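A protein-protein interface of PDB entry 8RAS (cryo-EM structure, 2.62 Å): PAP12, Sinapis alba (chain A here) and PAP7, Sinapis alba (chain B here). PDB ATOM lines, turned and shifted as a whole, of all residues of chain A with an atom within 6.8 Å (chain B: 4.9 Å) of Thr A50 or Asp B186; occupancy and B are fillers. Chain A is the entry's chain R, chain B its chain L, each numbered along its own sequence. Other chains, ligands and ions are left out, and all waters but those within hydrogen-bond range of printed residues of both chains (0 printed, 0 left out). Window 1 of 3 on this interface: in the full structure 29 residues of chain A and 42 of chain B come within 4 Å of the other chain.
Of chain B, only Asp B76 (3.9 Å), Asp B186 (3.8 Å) and Phe B187 (3.9 Å) come within 4 Å of Thr A50.
Asp B186 touches four residues of chain A.
Of the printed residues of chain A, Phe B187 touches Arg A49 (3.0 Å), Thr A50 (3.9 Å) and Leu A51 (3.7 Å).
Of the printed residues of chain B, Leu A51 touches Asp B76, Leu B183, Asp B186 and Phe B187.
Printed residues of chain A within 4 Å of Arg B182: Lys A53 (3.4 Å).
Gly B185 touches none of the printed residues of chain A.
The nearest printed residue of chain B that does not touch Thr A50 is Leu B183 (6.1 Å).
The nearest residue of chain A that does not touch Asp B186 is Arg A49 (4.6 Å).
The nearest printed residue of chain A that does not touch Asp B76 is Thr A52 (6.1 Å).
Among the printed residues, merely in contact across the chains: Arg A49 with Asp B76 (3.8 Å), Thr A50 with Asp B76 (3.9 Å), Thr A50 with Asp B186 (3.8 Å), Thr A50 with Phe B187 (3.9 Å), Leu A51 with Asp B76 (3.6 Å), Leu A51 with Leu B183 (3.9 Å), Leu A51 with Phe B187 (3.7 Å), Thr A52 with Asp B186 (3.5 Å), Lys A53 with Arg B182 (3.4 Å) and Lys A53 with Asp B186 (3.3 Å).
Of the 8 printed residues of chain B, 5 touch a printed residue of chain A.
Printed residues of chain B that touch a printed residue of chain A: Asp B76, Arg B182, Leu B183, Asp B186 and Phe B187.
Among the printed residues, no Asp or Glu carboxylate lies within 4 Å of a Lys or Arg side-chain nitrogen of the other chain.
O of Phe B187 sits at hydrogen-bond distance from NH1 of Arg A49 (3.0 Å).
O of Leu A51 lies close to OD2 of Asp B186 (2.8 Å).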
ATOM      1  N   ARG A  47      -8.992  13.220  22.597  1.00  0.00           N
ATOM      2  CA  ARG A  47      -8.525  11.863  22.838  1.00  0.00           C
ATOM      3  C   ARG A  47      -7.630  11.411  21.693  1.00  0.00           C
ATOM      4  O   ARG A  47      -8.033  11.453  20.527  1.00  0.00           O
ATOM      5  CB  ARG A  47      -9.708  10.906  22.993  1.00  0.00           C
ATOM      6  CG  ARG A  47      -9.303   9.469  23.263  1.00  0.00           C
ATOM      7  CD  ARG A  47     -10.511   8.549  23.283  1.00  0.00           C
ATOM      8  NE  ARG A  47     -11.162   8.473  21.982  1.00  0.00           N
ATOM      9  CZ  ARG A  47     -10.753   7.703  20.982  1.00  0.00           C
ATOM     10  NH1 ARG A  47      -9.689   6.925  21.100  1.00  0.00           N
ATOM     11  NH2 ARG A  47     -11.428   7.713  19.837  1.00  0.00           N
ATOM     12  N   ARG A  48      -6.417  10.982  22.029  1.00  0.00           N
ATOM     13  CA  ARG A  48      -5.495  10.460  21.034  1.00  0.00           C
ATOM     14  C   ARG A  48      -5.886   9.039  20.652  1.00  0.00           C
ATOM     15  O   ARG A  48      -6.258   8.230  21.506  1.00  0.00           O
ATOM     16  CB  ARG A  48      -4.060  10.483  21.564  1.00  0.00           C
ATOM     17  CG  ARG A  48      -3.369  11.831  21.443  1.00  0.00           C
ATOM     18  CD  ARG A  48      -3.740  12.750  22.595  1.00  0.00           C
ATOM     19  NE  ARG A  48      -3.073  14.043  22.503  1.00  0.00           N
ATOM     20  CZ  ARG A  48      -3.635  15.199  22.824  1.00  0.00           C
ATOM     21  NH1 ARG A  48      -4.883  15.262  23.260  1.00  0.00           N
ATOM     22  NH2 ARG A  48      -2.930  16.320  22.704  1.00  0.00           N
ATOM     23  N   ARG A  49      -5.802   8.739  19.358  1.00  0.00           N
ATOM     24  CA  ARG A  49      -6.149   7.414  18.865  1.00  0.00           C
ATOM     25  C   ARG A  49      -4.950   6.484  18.988  1.00  0.00           C
ATOM     26  O   ARG A  49      -3.849   6.814  18.539  1.00  0.00           O
ATOM     27  CB  ARG A  49      -6.619   7.492  17.414  1.00  0.00           C
ATOM     28  CG  ARG A  49      -7.978   8.151  17.239  1.00  0.00           C
ATOM     29  CD  ARG A  49      -8.304   8.361  15.771  1.00  0.00           C
ATOM     30  NE  ARG A  49      -9.284   9.422  15.571  1.00  0.00           N
ATOM     31  CZ  ARG A  49      -9.729   9.816  14.387  1.00  0.00           C
ATOM     32  NH1 ARG A  49      -9.304   9.256  13.267  1.00  0.00           N
ATOM     33  NH2 ARG A  49     -10.625  10.797  14.323  1.00  0.00           N
ATOM     34  N   THR A  50      -5.166   5.319  19.596  1.00  0.00           N
ATOM     35  CA  THR A  50      -4.104   4.357  19.839  1.00  0.00           C
ATOM     36  C   THR A  50      -4.542   2.974  19.377  1.00  0.00           C
ATOM     37  O   THR A  50      -5.730   2.705  19.185  1.00  0.00           O
ATOM     38  CB  THR A  50      -3.710   4.306  21.322  1.00  0.00           C
ATOM     39  OG1 THR A  50      -4.888   4.199  22.129  1.00  0.00           O
ATOM     40  CG2 THR A  50      -2.944   5.562  21.712  1.00  0.00           C
ATOM     41  N   LEU A  51      -3.551   2.097  19.198  1.00  0.00           N
ATOM     42  CA  LEU A  51      -3.825   0.754  18.696  1.00  0.00           C
ATOM     43  C   LEU A  51      -4.679  -0.046  19.672  1.00  0.00           C
ATOM     44  O   LEU A  51      -5.573  -0.789  19.253  1.00  0.00           O
ATOM     45  CB  LEU A  51      -2.509   0.028  18.411  1.00  0.00           C
ATOM     46  CG  LEU A  51      -2.599  -1.361  17.781  1.00  0.00           C
ATOM     47  CD1 LEU A  51      -3.602  -1.379  16.640  1.00  0.00           C
ATOM     48  CD2 LEU A  51      -1.232  -1.812  17.297  1.00  0.00           C
ATOM     49  N   THR A  52      -4.391   0.068  20.973  1.00  0.00           N
ATOM     50  CA  THR A  52      -5.118  -0.592  22.069  1.00  0.00           C
ATOM     51  C   THR A  52      -5.371  -2.079  21.804  1.00  0.00           C
ATOM     52  O   THR A  52      -6.276  -2.683  22.392  1.00  0.00           O
ATOM     53  CB  THR A  52      -6.429   0.144  22.408  1.00  0.00           C
ATOM     54  OG1 THR A  52      -6.863  -0.234  23.721  1.00  0.00           O
ATOM     55  CG2 THR A  52      -7.553  -0.145  21.410  1.00  0.00           C
ATOM     56  N   LYS A  53      -4.548  -2.701  20.963  1.00  0.00           N
ATOM     57  CA  LYS A  53      -4.695  -4.111  20.638  1.00  0.00           C
ATOM     58  C   LYS A  53      -3.314  -4.702  20.391  1.00  0.00           C
ATOM     59  O   LYS A  53      -2.326  -3.982  20.228  1.00  0.00           O
ATOM     60  CB  LYS A  53      -5.601  -4.322  19.420  1.00  0.00           C
ATOM     61  CG  LYS A  53      -7.080  -4.421  19.750  1.00  0.00           C
ATOM     62  CD  LYS A  53      -7.882  -4.896  18.548  1.00  0.00           C
ATOM     63  CE  LYS A  53      -9.374  -4.722  18.772  1.00  0.00           C
ATOM     64  NZ  LYS A  53      -9.884  -5.639  19.826  1.00  0.00           N
ATOM     65  N   ASP B  76       0.163   8.064  16.001  1.00  0.00           N
ATOM     66  CA  ASP B  76       0.713   6.890  16.659  1.00  0.00           C
ATOM     67  C   ASP B  76       1.526   6.082  15.652  1.00  0.00           C
ATOM     68  O   ASP B  76       1.010   5.745  14.577  1.00  0.00           O
ATOM     69  CB  ASP B  76      -0.413   6.038  17.242  1.00  0.00           C
ATOM     70  CG  ASP B  76       0.091   4.954  18.171  1.00  0.00           C
ATOM     71  OD1 ASP B  76       1.140   5.159  18.817  1.00  0.00           O
ATOM     72  OD2 ASP B  76      -0.564   3.895  18.258  1.00  0.00           O
ATOM     73  N   ARG B 182      -9.926  -5.359  12.248  1.00  0.00           N
ATOM     74  CA  ARG B 182     -10.033  -5.472  13.698  1.00  0.00           C
ATOM     75  C   ARG B 182      -9.029  -4.557  14.387  1.00  0.00           C
ATOM     76  O   ARG B 182      -9.317  -3.989  15.447  1.00  0.00           O
ATOM     77  CB  ARG B 182      -9.825  -6.924  14.130  1.00  0.00           C
ATOM     78  CG  ARG B 182     -10.011  -7.161  15.619  1.00  0.00           C
ATOM     79  CD  ARG B 182     -10.040  -8.644  15.948  1.00  0.00           C
ATOM     80  NE  ARG B 182     -10.038  -8.883  17.386  1.00  0.00           N
ATOM     81  CZ  ARG B 182     -11.124  -8.895  18.147  1.00  0.00           C
ATOM     82  NH1 ARG B 182     -12.327  -8.685  17.637  1.00  0.00           N
ATOM     83  NH2 ARG B 182     -11.000  -9.124  19.451  1.00  0.00           N
ATOM     84  N   LEU B 183      -7.845  -4.400  13.796  1.00  0.00           N
ATOM     85  CA  LEU B 183      -6.835  -3.484  14.310  1.00  0.00           C
ATOM     86  C   LEU B 183      -7.014  -2.069  13.773  1.00  0.00           C
ATOM     87  O   LEU B 183      -6.873  -1.101  14.527  1.00  0.00           O
ATOM     88  CB  LEU B 183      -5.434  -3.991  13.961  1.00  0.00           C
ATOM     89  CG  LEU B 183      -5.233  -5.507  13.962  1.00  0.00           C
ATOM     90  CD1 LEU B 183      -3.887  -5.861  13.354  1.00  0.00           C
ATOM     91  CD2 LEU B 183      -5.350  -6.061  15.371  1.00  0.00           C
ATOM     92  N   TYR B 184      -7.317  -1.931  12.480  1.00  0.00           N
ATOM     93  CA  TYR B 184      -7.490  -0.605  11.899  1.00  0.00           C
ATOM     94  C   TYR B 184      -8.744   0.081  12.422  1.00  0.00           C
ATOM     95  O   TYR B 184      -8.808   1.314  12.450  1.00  0.00           O
ATOM     96  CB  TYR B 184      -7.538  -0.698  10.375  1.00  0.00           C
ATOM     97  CG  TYR B 184      -7.556   0.643   9.678  1.00  0.00           C
ATOM     98  CD1 TYR B 184      -6.378   1.326   9.418  1.00  0.00           C
ATOM     99  CD2 TYR B 184      -8.752   1.223   9.278  1.00  0.00           C
ATOM    100  CE1 TYR B 184      -6.388   2.550   8.783  1.00  0.00           C
ATOM    101  CE2 TYR B 184      -8.772   2.447   8.642  1.00  0.00           C
ATOM    102  CZ  TYR B 184      -7.588   3.106   8.397  1.00  0.00           C
ATOM    103  OH  TYR B 184      -7.602   4.325   7.762  1.00  0.00           O
ATOM    104  N   GLY B 185      -9.745  -0.694  12.838  1.00  0.00           N
ATOM    105  CA  GLY B 185     -10.964  -0.117  13.373  1.00  0.00           C
ATOM    106  C   GLY B 185     -10.781   0.645  14.667  1.00  0.00           C
ATOM    107  O   GLY B 185     -11.695   1.373  15.070  1.00  0.00           O
ATOM    108  N   ASP B 186      -9.634   0.494  15.326  1.00  0.00           N
ATOM    109  CA  ASP B 186      -9.351   1.241  16.544  1.00  0.00           C
ATOM    110  C   ASP B 186      -8.931   2.678  16.272  1.00  0.00           C
ATOM    111  O   ASP B 186      -8.876   3.477  17.211  1.00  0.00           O
ATOM    112  CB  ASP B 186      -8.264   0.532  17.353  1.00  0.00           C
ATOM    113  CG  ASP B 186      -8.802  -0.640  18.147  1.00  0.00           C
ATOM    114  OD1 ASP B 186      -9.945  -0.546  18.644  1.00  0.00           O
ATOM    115  OD2 ASP B 186      -8.088  -1.654  18.273  1.00  0.00           O
ATOM    116  N   PHE B 187      -8.633   3.023  15.022  1.00  0.00           N
ATOM    117  CA  PHE B 187      -8.300   4.388  14.646  1.00  0.00           C
ATOM    118  C   PHE B 187      -9.456   5.111  13.971  1.00  0.00           C
ATOM    119  O   PHE B 187      -9.297   6.268  13.572  1.00  0.00           O
ATOM    120  CB  PHE B 187      -7.076   4.400  13.728  1.00  0.00           C
ATOM    121  CG  PHE B 187      -5.832   3.866  14.375  1.00  0.00           C
ATOM    122  CD1 PHE B 187      -5.519   2.519  14.299  1.00  0.00           C
ATOM    123  CD2 PHE B 187      -4.978   4.709  15.064  1.00  0.00           C
ATOM    124  CE1 PHE B 187      -4.376   2.026  14.892  1.00  0.00           C
ATOM    125  CE2 PHE B 187      -3.834   4.219  15.660  1.00  0.00           C
ATOM    126  CZ  PHE B 187      -3.533   2.878  15.573  1.00  0.00           C
ATOM    127  N   LEU B 188     -10.602   4.456  13.819  1.00  0.00           N
ATOM    128  CA  LEU B 188     -11.781   5.138  13.322  1.00  0.00           C
ATOM    129  C   LEU B 188     -12.318   6.090  14.389  1.00  0.00           C
ATOM    130  O   LEU B 188     -12.194   5.823  15.587  1.00  0.00           O
ATOM    131  CB  LEU B 188     -12.861   4.132  12.935  1.00  0.00           C
ATOM    132  CG  LEU B 188     -12.473   3.068  11.911  1.00  0.00           C
ATOM    133  CD1 LEU B 188     -13.675   2.210  11.555  1.00  0.00           C
ATOM    134  CD2 LEU B 188     -11.882   3.710  10.670  1.00  0.00           C
